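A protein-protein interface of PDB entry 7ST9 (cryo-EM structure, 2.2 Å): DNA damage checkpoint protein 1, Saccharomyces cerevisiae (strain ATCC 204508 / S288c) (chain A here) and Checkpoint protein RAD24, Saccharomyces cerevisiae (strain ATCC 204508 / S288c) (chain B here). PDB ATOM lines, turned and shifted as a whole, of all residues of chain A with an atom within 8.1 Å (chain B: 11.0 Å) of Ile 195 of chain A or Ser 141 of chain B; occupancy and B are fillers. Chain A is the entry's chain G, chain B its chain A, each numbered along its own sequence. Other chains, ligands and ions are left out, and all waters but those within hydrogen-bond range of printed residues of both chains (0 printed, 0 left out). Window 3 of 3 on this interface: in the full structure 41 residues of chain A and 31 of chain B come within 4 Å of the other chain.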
ATOM      1  N   GLN A  87      35.916  -0.315  11.522  1.00  0.00           N
ATOM      2  CA  GLN A  87      36.507   0.365  12.667  1.00  0.00           C
ATOM      3  C   GLN A  87      37.445  -0.583  13.399  1.00  0.00           C
ATOM      4  O   GLN A  87      37.048  -1.692  13.769  1.00  0.00           O
ATOM      5  CB  GLN A  87      35.412   0.869  13.616  1.00  0.00           C
ATOM      6  CG  GLN A  87      35.920   1.467  14.913  1.00  0.00           C
ATOM      7  CD  GLN A  87      34.806   2.065  15.752  1.00  0.00           C
ATOM      8  OE1 GLN A  87      34.516   1.591  16.849  1.00  0.00           O
ATOM      9  NE2 GLN A  87      34.173   3.110  15.234  1.00  0.00           N
ATOM     10  N   TYR A 191      34.404  13.978  15.404  1.00  0.00           N
ATOM     11  CA  TYR A 191      34.083  12.564  15.549  1.00  0.00           C
ATOM     12  C   TYR A 191      32.620  12.402  15.940  1.00  0.00           C
ATOM     13  O   TYR A 191      32.161  13.014  16.910  1.00  0.00           O
ATOM     14  CB  TYR A 191      34.984  11.908  16.596  1.00  0.00           C
ATOM     15  CG  TYR A 191      34.721  10.434  16.796  1.00  0.00           C
ATOM     16  CD1 TYR A 191      34.763   9.550  15.727  1.00  0.00           C
ATOM     17  CD2 TYR A 191      34.435   9.925  18.055  1.00  0.00           C
ATOM     18  CE1 TYR A 191      34.526   8.201  15.906  1.00  0.00           C
ATOM     19  CE2 TYR A 191      34.196   8.578  18.244  1.00  0.00           C
ATOM     20  CZ  TYR A 191      34.242   7.721  17.166  1.00  0.00           C
ATOM     21  OH  TYR A 191      34.004   6.379  17.348  1.00  0.00           O
ATOM     22  N   ASP A 192      31.900  11.576  15.187  1.00  0.00           N
ATOM     23  CA  ASP A 192      30.509  11.232  15.485  1.00  0.00           C
ATOM     24  C   ASP A 192      30.439   9.743  15.796  1.00  0.00           C
ATOM     25  O   ASP A 192      30.451   8.913  14.869  1.00  0.00           O
ATOM     26  CB  ASP A 192      29.594  11.583  14.313  1.00  0.00           C
ATOM     27  CG  ASP A 192      28.137  11.693  14.722  1.00  0.00           C
ATOM     28  OD1 ASP A 192      27.844  11.579  15.930  1.00  0.00           O
ATOM     29  OD2 ASP A 192      27.284  11.892  13.831  1.00  0.00           O
ATOM     30  N   PRO A 193      30.373   9.347  17.068  1.00  0.00           N
ATOM     31  CA  PRO A 193      30.411   7.917  17.393  1.00  0.00           C
ATOM     32  C   PRO A 193      29.253   7.155  16.766  1.00  0.00           C
ATOM     33  O   PRO A 193      28.133   7.658  16.654  1.00  0.00           O
ATOM     34  CB  PRO A 193      30.330   7.893  18.924  1.00  0.00           C
ATOM     35  CG  PRO A 193      30.747   9.250  19.361  1.00  0.00           C
ATOM     36  CD  PRO A 193      30.324  10.186  18.279  1.00  0.00           C
ATOM     37  N   ILE A 194      29.541   5.921  16.360  1.00  0.00           N
ATOM     38  CA  ILE A 194      28.543   5.006  15.821  1.00  0.00           C
ATOM     39  C   ILE A 194      28.080   4.099  16.954  1.00  0.00           C
ATOM     40  O   ILE A 194      28.904   3.538  17.686  1.00  0.00           O
ATOM     41  CB  ILE A 194      29.109   4.194  14.642  1.00  0.00           C
ATOM     42  CG1 ILE A 194      27.982   3.752  13.708  1.00  0.00           C
ATOM     43  CG2 ILE A 194      29.902   2.988  15.134  1.00  0.00           C
ATOM     44  CD1 ILE A 194      28.467   3.134  12.413  1.00  0.00           C
ATOM     45  N   ILE A 195      26.762   3.971  17.112  1.00  0.00           N
ATOM     46  CA  ILE A 195      26.174   3.257  18.237  1.00  0.00           C
ATOM     47  C   ILE A 195      25.373   2.041  17.793  1.00  0.00           C
ATOM     48  O   ILE A 195      24.649   1.457  18.598  1.00  0.00           O
ATOM     49  CB  ILE A 195      25.300   4.197  19.090  1.00  0.00           C
ATOM     50  CG1 ILE A 195      24.009   4.544  18.343  1.00  0.00           C
ATOM     51  CG2 ILE A 195      26.076   5.457  19.448  1.00  0.00           C
ATOM     52  CD1 ILE A 195      23.262   5.728  18.919  1.00  0.00           C
ATOM     53  N   ILE A 196      25.488   1.640  16.526  1.00  0.00           N
ATOM     54  CA  ILE A 196      24.736   0.482  16.050  1.00  0.00           C
ATOM     55  C   ILE A 196      25.126  -0.764  16.835  1.00  0.00           C
ATOM     56  O   ILE A 196      24.271  -1.583  17.197  1.00  0.00           O
ATOM     57  CB  ILE A 196      24.948   0.290  14.536  1.00  0.00           C
ATOM     58  CG1 ILE A 196      24.026  -0.806  13.992  1.00  0.00           C
ATOM     59  CG2 ILE A 196      26.399  -0.054  14.233  1.00  0.00           C
ATOM     60  CD1 ILE A 196      22.550  -0.506  14.142  1.00  0.00           C
ATOM     61  N   ASN A 197      26.421  -0.926  17.111  1.00  0.00           N
ATOM     62  CA  ASN A 197      26.875  -2.104  17.843  1.00  0.00           C
ATOM     63  C   ASN A 197      26.275  -2.148  19.242  1.00  0.00           C
ATOM     64  O   ASN A 197      25.859  -3.213  19.711  1.00  0.00           O
ATOM     65  CB  ASN A 197      28.403  -2.123  17.912  1.00  0.00           C
ATOM     66  CG  ASN A 197      28.977  -0.863  18.527  1.00  0.00           C
ATOM     67  OD1 ASN A 197      29.171   0.142  17.844  1.00  0.00           O
ATOM     68  ND2 ASN A 197      29.253  -0.912  19.824  1.00  0.00           N
ATOM     69  N   LEU A 198      26.225  -1.003  19.927  1.00  0.00           N
ATOM     70  CA  LEU A 198      25.668  -0.978  21.277  1.00  0.00           C
ATOM     71  C   LEU A 198      24.193  -1.361  21.274  1.00  0.00           C
ATOM     72  O   LEU A 198      23.745  -2.145  22.119  1.00  0.00           O
ATOM     73  CB  LEU A 198      25.854   0.410  21.893  1.00  0.00           C
ATOM     74  CG  LEU A 198      27.194   0.773  22.548  1.00  0.00           C
ATOM     75  CD1 LEU A 198      26.977   1.873  23.575  1.00  0.00           C
ATOM     76  CD2 LEU A 198      27.885  -0.422  23.193  1.00  0.00           C
ATOM     77  N   LYS A 199      23.419  -0.811  20.334  1.00  0.00           N
ATOM     78  CA  LYS A 199      21.997  -1.136  20.273  1.00  0.00           C
ATOM     79  C   LYS A 199      21.785  -2.605  19.933  1.00  0.00           C
ATOM     80  O   LYS A 199      20.917  -3.266  20.518  1.00  0.00           O
ATOM     81  CB  LYS A 199      21.287  -0.244  19.251  1.00  0.00           C
ATOM     82  CG  LYS A 199      21.794   1.199  19.187  1.00  0.00           C
ATOM     83  CD  LYS A 199      20.660   2.213  19.274  1.00  0.00           C
ATOM     84  CE  LYS A 199      20.106   2.544  17.899  1.00  0.00           C
ATOM     85  NZ  LYS A 199      18.892   3.403  17.980  1.00  0.00           N
ATOM     86  N   TYR A 200      22.571  -3.136  18.993  1.00  0.00           N
ATOM     87  CA  TYR A 200      22.457  -4.550  18.657  1.00  0.00           C
ATOM     88  C   TYR A 200      22.793  -5.426  19.856  1.00  0.00           C
ATOM     89  O   TYR A 200      22.113  -6.425  20.112  1.00  0.00           O
ATOM     90  CB  TYR A 200      23.369  -4.885  17.476  1.00  0.00           C
ATOM     91  CG  TYR A 200      22.707  -4.752  16.121  1.00  0.00           C
ATOM     92  CD1 TYR A 200      21.692  -3.828  15.905  1.00  0.00           C
ATOM     93  CD2 TYR A 200      23.099  -5.553  15.057  1.00  0.00           C
ATOM     94  CE1 TYR A 200      21.088  -3.707  14.668  1.00  0.00           C
ATOM     95  CE2 TYR A 200      22.502  -5.438  13.817  1.00  0.00           C
ATOM     96  CZ  TYR A 200      21.497  -4.514  13.629  1.00  0.00           C
ATOM     97  OH  TYR A 200      20.899  -4.399  12.396  1.00  0.00           O
ATOM     98  N   LYS A 201      23.837  -5.066  20.606  1.00  0.00           N
ATOM     99  CA  LYS A 201      24.206  -5.845  21.782  1.00  0.00           C
ATOM    100  C   LYS A 201      23.112  -5.797  22.841  1.00  0.00           C
ATOM    101  O   LYS A 201      22.792  -6.818  23.459  1.00  0.00           O
ATOM    102  CB  LYS A 201      25.527  -5.331  22.355  1.00  0.00           C
ATOM    103  CG  LYS A 201      26.724  -5.584  21.457  1.00  0.00           C
ATOM    104  CD  LYS A 201      27.323  -6.958  21.707  1.00  0.00           C
ATOM    105  CE  LYS A 201      28.627  -7.147  20.949  1.00  0.00           C
ATOM    106  NZ  LYS A 201      28.544  -6.642  19.552  1.00  0.00           N
ATOM    107  N   ARG A 202      22.532  -4.617  23.069  1.00  0.00           N
ATOM    108  CA  ARG A 202      21.457  -4.502  24.049  1.00  0.00           C
ATOM    109  C   ARG A 202      20.258  -5.351  23.642  1.00  0.00           C
ATOM    110  O   ARG A 202      19.679  -6.067  24.468  1.00  0.00           O
ATOM    111  CB  ARG A 202      21.054  -3.034  24.212  1.00  0.00           C
ATOM    112  CG  ARG A 202      20.147  -2.703  25.410  1.00  0.00           C
ATOM    113  CD  ARG A 202      20.256  -3.678  26.583  1.00  0.00           C
ATOM    114  NE  ARG A 202      21.574  -3.660  27.208  1.00  0.00           N
ATOM    115  CZ  ARG A 202      22.042  -2.659  27.941  1.00  0.00           C
ATOM    116  NH1 ARG A 202      21.327  -1.569  28.162  1.00  0.00           N
ATOM    117  NH2 ARG A 202      23.257  -2.758  28.471  1.00  0.00           N
ATOM    118  N   LEU A 236      28.938  -3.072  27.252  1.00  0.00           N
ATOM    119  CA  LEU A 236      27.881  -2.068  27.227  1.00  0.00           C
ATOM    120  C   LEU A 236      28.016  -1.098  28.395  1.00  0.00           C
ATOM    121  O   LEU A 236      27.853   0.116  28.225  1.00  0.00           O
ATOM    122  CB  LEU A 236      26.513  -2.751  27.248  1.00  0.00           C
ATOM    123  CG  LEU A 236      25.882  -2.968  25.871  1.00  0.00           C
ATOM    124  CD1 LEU A 236      24.911  -4.142  25.882  1.00  0.00           C
ATOM    125  CD2 LEU A 236      25.179  -1.701  25.411  1.00  0.00           C
ATOM    126  N   LEU A 240      30.853   4.654  26.646  1.00  0.00           N
ATOM    127  CA  LEU A 240      30.536   6.020  27.044  1.00  0.00           C
ATOM    128  C   LEU A 240      29.065   6.365  26.854  1.00  0.00           C
ATOM    129  O   LEU A 240      28.626   7.409  27.349  1.00  0.00           O
ATOM    130  CB  LEU A 240      31.397   7.006  26.252  1.00  0.00           C
ATOM    131  CG  LEU A 240      32.912   6.814  26.359  1.00  0.00           C
ATOM    132  CD1 LEU A 240      33.637   7.767  25.424  1.00  0.00           C
ATOM    133  CD2 LEU A 240      33.383   7.004  27.793  1.00  0.00           C
ATOM    134  N   PHE A 241      28.300   5.527  26.157  1.00  0.00           N
ATOM    135  CA  PHE A 241      26.894   5.787  25.890  1.00  0.00           C
ATOM    136  C   PHE A 241      26.068   4.569  26.280  1.00  0.00           C
ATOM    137  O   PHE A 241      26.558   3.437  26.299  1.00  0.00           O
ATOM    138  CB  PHE A 241      26.656   6.131  24.413  1.00  0.00           C
ATOM    139  CG  PHE A 241      27.661   7.092  23.845  1.00  0.00           C
ATOM    140  CD1 PHE A 241      28.879   6.638  23.365  1.00  0.00           C
ATOM    141  CD2 PHE A 241      27.390   8.448  23.793  1.00  0.00           C
ATOM    142  CE1 PHE A 241      29.806   7.521  22.844  1.00  0.00           C
ATOM    143  CE2 PHE A 241      28.313   9.334  23.272  1.00  0.00           C
ATOM    144  CZ  PHE A 241      29.523   8.869  22.798  1.00  0.00           C
ATOM    145  N   ASN A 242      24.801   4.819  26.594  1.00  0.00           N
ATOM    146  CA  ASN A 242      23.881   3.758  26.989  1.00  0.00           C
ATOM    147  C   ASN A 242      23.758   2.708  25.889  1.00  0.00           C
ATOM    148  O   ASN A 242      22.733   2.619  25.214  1.00  0.00           O
ATOM    149  CB  ASN A 242      22.505   4.339  27.318  1.00  0.00           C
ATOM    150  CG  ASN A 242      21.590   3.331  27.982  1.00  0.00           C
ATOM    151  OD1 ASN A 242      22.041   2.465  28.732  1.00  0.00           O
ATOM    152  ND2 ASN A 242      20.295   3.437  27.709  1.00  0.00           N
ATOM    153  N   LEU A 395      26.114  -6.639  11.681  1.00  0.00           N
ATOM    154  CA  LEU A 395      27.295  -6.292  12.459  1.00  0.00           C
ATOM    155  C   LEU A 395      28.204  -7.508  12.580  1.00  0.00           C
ATOM    156  O   LEU A 395      27.727  -8.638  12.700  1.00  0.00           O
ATOM    157  CB  LEU A 395      26.901  -5.790  13.853  1.00  0.00           C
ATOM    158  CG  LEU A 395      28.019  -5.615  14.883  1.00  0.00           C
ATOM    159  CD1 LEU A 395      28.922  -4.453  14.506  1.00  0.00           C
ATOM    160  CD2 LEU A 395      27.428  -5.413  16.267  1.00  0.00           C
ATOM    161  N   VAL A 408      30.304  -3.088   9.828  1.00  0.00           N
ATOM    162  CA  VAL A 408      28.859  -2.949   9.702  1.00  0.00           C
ATOM    163  C   VAL A 408      28.531  -2.798   8.225  1.00  0.00           C
ATOM    164  O   VAL A 408      29.146  -1.982   7.530  1.00  0.00           O
ATOM    165  CB  VAL A 408      28.328  -1.746  10.505  1.00  0.00           C
ATOM    166  CG1 VAL A 408      26.809  -1.683  10.426  1.00  0.00           C
ATOM    167  CG2 VAL A 408      28.789  -1.827  11.951  1.00  0.00           C
ATOM    168  N   SER B 134      12.808   3.683   9.986  1.00  0.00           N
ATOM    169  CA  SER B 134      13.666   2.610  10.464  1.00  0.00           C
ATOM    170  C   SER B 134      13.056   1.940  11.690  1.00  0.00           C
ATOM    171  O   SER B 134      12.394   2.579  12.512  1.00  0.00           O
ATOM    172  CB  SER B 134      15.055   3.150  10.802  1.00  0.00           C
ATOM    173  OG  SER B 134      14.989   4.099  11.853  1.00  0.00           O
ATOM    174  N   GLY B 136      13.958   1.236  14.549  1.00  0.00           N
ATOM    175  CA  GLY B 136      14.891   1.515  15.629  1.00  0.00           C
ATOM    176  C   GLY B 136      16.313   1.119  15.302  1.00  0.00           C
ATOM    177  O   GLY B 136      17.052   0.675  16.189  1.00  0.00           O
ATOM    178  N   THR B 137      16.715   1.270  14.041  1.00  0.00           N
ATOM    179  CA  THR B 137      18.055   0.919  13.593  1.00  0.00           C
ATOM    180  C   THR B 137      18.612   2.043  12.733  1.00  0.00           C
ATOM    181  O   THR B 137      17.901   2.608  11.896  1.00  0.00           O
ATOM    182  CB  THR B 137      18.056  -0.392  12.797  1.00  0.00           C
ATOM    183  OG1 THR B 137      16.989  -0.378  11.841  1.00  0.00           O
ATOM    184  CG2 THR B 137      17.885  -1.583  13.727  1.00  0.00           C
ATOM    185  N   SER B 138      19.886   2.358  12.942  1.00  0.00           N
ATOM    186  CA  SER B 138      20.563   3.401  12.184  1.00  0.00           C
ATOM    187  C   SER B 138      22.038   3.368  12.547  1.00  0.00           C
ATOM    188  O   SER B 138      22.421   2.879  13.614  1.00  0.00           O
ATOM    189  CB  SER B 138      19.969   4.786  12.465  1.00  0.00           C
ATOM    190  OG  SER B 138      20.146   5.148  13.824  1.00  0.00           O
ATOM    191  N   PHE B 139      22.864   3.897  11.643  1.00  0.00           N
ATOM    192  CA  PHE B 139      24.303   3.915  11.875  1.00  0.00           C
ATOM    193  C   PHE B 139      24.638   4.668  13.158  1.00  0.00           C
ATOM    194  O   PHE B 139      25.168   4.091  14.114  1.00  0.00           O
ATOM    195  CB  PHE B 139      25.015   4.545  10.676  1.00  0.00           C
ATOM    196  CG  PHE B 139      25.387   3.558   9.604  1.00  0.00           C
ATOM    197  CD1 PHE B 139      24.522   2.535   9.253  1.00  0.00           C
ATOM    198  CD2 PHE B 139      26.601   3.659   8.944  1.00  0.00           C
ATOM    199  CE1 PHE B 139      24.862   1.628   8.267  1.00  0.00           C
ATOM    200  CE2 PHE B 139      26.945   2.755   7.955  1.00  0.00           C
ATOM    201  CZ  PHE B 139      26.074   1.739   7.618  1.00  0.00           C
ATOM    202  N   ARG B 140      24.318   5.957  13.201  1.00  0.00           N
ATOM    203  CA  ARG B 140      24.637   6.820  14.327  1.00  0.00           C
ATOM    204  C   ARG B 140      23.352   7.309  14.993  1.00  0.00           C
ATOM    205  O   ARG B 140      22.238   6.997  14.563  1.00  0.00           O
ATOM    206  CB  ARG B 140      25.502   7.995  13.866  1.00  0.00           C
ATOM    207  CG  ARG B 140      26.833   7.574  13.261  1.00  0.00           C
ATOM    208  CD  ARG B 140      27.561   8.749  12.633  1.00  0.00           C
ATOM    209  NE  ARG B 140      28.844   8.355  12.063  1.00  0.00           N
ATOM    210  CZ  ARG B 140      29.592   9.131  11.290  1.00  0.00           C
ATOM    211  NH1 ARG B 140      29.212  10.357  10.966  1.00  0.00           N
ATOM    212  NH2 ARG B 140      30.749   8.666  10.830  1.00  0.00           N
ATOM    213  N   SER B 141      23.523   8.089  16.063  1.00  0.00           N
ATOM    214  CA  SER B 141      22.372   8.605  16.796  1.00  0.00           C
ATOM    215  C   SER B 141      21.523   9.516  15.920  1.00  0.00           C
ATOM    216  O   SER B 141      20.288   9.469  15.973  1.00  0.00           O
ATOM    217  CB  SER B 141      22.840   9.350  18.046  1.00  0.00           C
ATOM    218  OG  SER B 141      21.743   9.696  18.874  1.00  0.00           O
ATOM    219  N   THR B 142      22.164  10.352  15.109  1.00  0.00           N
ATOM    220  CA  THR B 142      21.438  11.277  14.259  1.00  0.00           C
ATOM    221  C   THR B 142      20.655  10.516  13.191  1.00  0.00           C
ATOM    222  O   THR B 142      20.980   9.371  12.866  1.00  0.00           O
ATOM    223  CB  THR B 142      22.403  12.258  13.596  1.00  0.00           C
ATOM    224  OG1 THR B 142      23.486  11.537  12.995  1.00  0.00           O
ATOM    225  CG2 THR B 142      22.955  13.238  14.621  1.00  0.00           C
ATOM    226  N   PRO B 143      19.610  11.133  12.630  1.00  0.00           N
ATOM    227  CA  PRO B 143      18.801  10.443  11.613  1.00  0.00           C
ATOM    228  C   PRO B 143      19.538  10.152  10.315  1.00  0.00           C
ATOM    229  O   PRO B 143      18.917   9.631   9.381  1.00  0.00           O
ATOM    230  CB  PRO B 143      17.634  11.415  11.375  1.00  0.00           C
ATOM    231  CG  PRO B 143      18.130  12.741  11.824  1.00  0.00           C
ATOM    232  CD  PRO B 143      19.078  12.469  12.949  1.00  0.00           C
ATOM    233  N   ASN B 144      20.832  10.464  10.214  1.00  0.00           N
ATOM    234  CA  ASN B 144      21.629  10.162   9.026  1.00  0.00           C
ATOM    235  C   ASN B 144      21.040  10.849   7.789  1.00  0.00           C
ATOM    236  O   ASN B 144      20.555  10.217   6.849  1.00  0.00           O
ATOM    237  CB  ASN B 144      21.732   8.646   8.817  1.00  0.00           C
ATOM    238  CG  ASN B 144      22.310   7.930  10.022  1.00  0.00           C
ATOM    239  OD1 ASN B 144      23.001   8.532  10.844  1.00  0.00           O
ATOM    240  ND2 ASN B 144      22.030   6.638  10.132  1.00  0.00           N
ATOM    241  N   GLU B 145      21.099  12.181   7.824  1.00  0.00           N
ATOM    242  CA  GLU B 145      20.565  12.990   6.736  1.00  0.00           C
ATOM    243  C   GLU B 145      21.459  12.877   5.508  1.00  0.00           C
ATOM    244  O   GLU B 145      22.358  13.699   5.302  1.00  0.00           O
ATOM    245  CB  GLU B 145      20.437  14.453   7.172  1.00  0.00           C
ATOM    246  CG  GLU B 145      19.743  15.348   6.157  1.00  0.00           C
ATOM    247  CD  GLU B 145      19.778  16.812   6.552  1.00  0.00           C
ATOM    248  OE1 GLU B 145      20.327  17.126   7.629  1.00  0.00           O
ATOM    249  OE2 GLU B 145      19.258  17.649   5.783  1.00  0.00           O
ATOM    250  N   HIS B 146      21.214  11.856   4.691  1.00  0.00           N
ATOM    251  CA  HIS B 146      21.985  11.564   3.486  1.00  0.00           C
ATOM    252  C   HIS B 146      21.049  11.422   2.292  1.00  0.00           C
ATOM    253  O   HIS B 146      21.098  10.449   1.537  1.00  0.00           O
ATOM    254  CB  HIS B 146      22.824  10.304   3.675  1.00  0.00           C
ATOM    255  CG  HIS B 146      23.954  10.474   4.642  1.00  0.00           C
ATOM    256  ND1 HIS B 146      23.763  10.541   6.005  1.00  0.00           N
ATOM    257  CD2 HIS B 146      25.288  10.589   4.443  1.00  0.00           C
ATOM    258  CE1 HIS B 146      24.930  10.691   6.604  1.00  0.00           C
ATOM    259  NE2 HIS B 146      25.872  10.723   5.679  1.00  0.00           N
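The backbone carbonyl oxygen (O) of Phe 139 of chain B sits at hydrogen-bond distance from the backbone NH (N) of Ile 195 of chain A, 3.4 Å away.
The backbone carbonyl oxygen (O) of Phe 139 of chain B sits at hydrogen-bond distance from the backbone NH (N) of Ile 196 of chain A (3.5 Å).
NH1 of Arg 140 of chain B is in salt-bridge range of OD2 of Asp 192 of chain A, at 3.8 Å.
The side-chain hydroxyl (OG) of Ser 134 of chain B sits close to the backbone carbonyl oxygen (O) of Thr 137 of chain B (3.3 Å).
The side-chain hydroxyl of Ser 138 of chain B sits at hydrogen-bond distance from the backbone carbonyl oxygen of Arg 140 of chain B, at 2.9 Å.
The side-chain amide nitrogen (ND2) of Asn 144 of chain B lies close to the backbone NH (N) of Phe 139 of chain B (3.2 Å).
The backbone carbonyl oxygen of Thr 142 of chain B sits close to the side-chain amide oxygen of Asn 144 of chain B, 3.0 Å away.
The side-chain amide oxygen of Asn 197 of chain A sits close to the backbone carbonyl oxygen of Ile 194 of chain A, at 3.4 Å.
Among the printed residues, pairs that only touch across the chains: Ile 194 of chain A with Phe 139 of chain B (2.9 Å), Ile 196 of chain A with Ser 138 of chain B (3.4 Å), Pro 193 of chain A with Arg 140 of chain B (3.6 Å), Ile 195 of chain A with Ser 141 of chain B (3.7 Å), Lys 199 of chain A with Gly 136 of chain B (3.7 Å), Asp 192 of chain A with Thr 142 of chain B (3.9 Å) and Tyr 200 of chain A with Thr 137 of chain B (3.96 Å).
Of chain B, only Phe 139 and Ser 141 come within 4 Å of Ile 195 of chain A.
Of chain B, only Arg 140 (3.6 Å) comes within 4 Å of Pro 193 of chain A.
Ile 196 of chain A touches two residues of chain B.
No residue of chain B comes within 4 Å of Leu 198 of chain A.
Printed residues of chain A within 4 Å of Arg 140 of chain B: Asp 192 (3.3 Å) and Pro 193 (3.6 Å).
Of the printed residues of chain A, Thr 137 of chain B touches Tyr 200.
Printed residues of chain A within 4 Å of Thr 142 of chain B: Asp 192.
Of the printed residues of chain B, Tyr 200 of chain A touches Thr 137 (3.96 Å).
Printed residues of chain A within 4 Å of Ser 138 of chain B: Ile 196 (3.4 Å).
Val 408 of chain A touches none of the printed residues of chain B.
Leu 240 of chain A touches none of the printed residues of chain B.
The nearest printed residue of chain A that does not touch Gly 136 of chain B is Ile 196 of chain A (6.0 Å).
Hydrophobic or aromatic side chains of chain B within 4 Å of the printed part of chain A: Phe 139.
Of the 19 printed residues of chain A, 7 touch a printed residue of chain B.
Printed residues of chain A that touch a printed residue of chain B: Asp 192, Pro 193, Ile 194, Ile 195, Ile 196, Lys 199 and Tyr 200.
Among the printed residues, 10 pairs touch across the chains.
Among the printed residues, Asp or Glu carboxylates within 4 Å of a Lys or Arg side-chain nitrogen of the other chain: Asp 192 of chain A with Arg 140 of chain B (3.8 Å).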
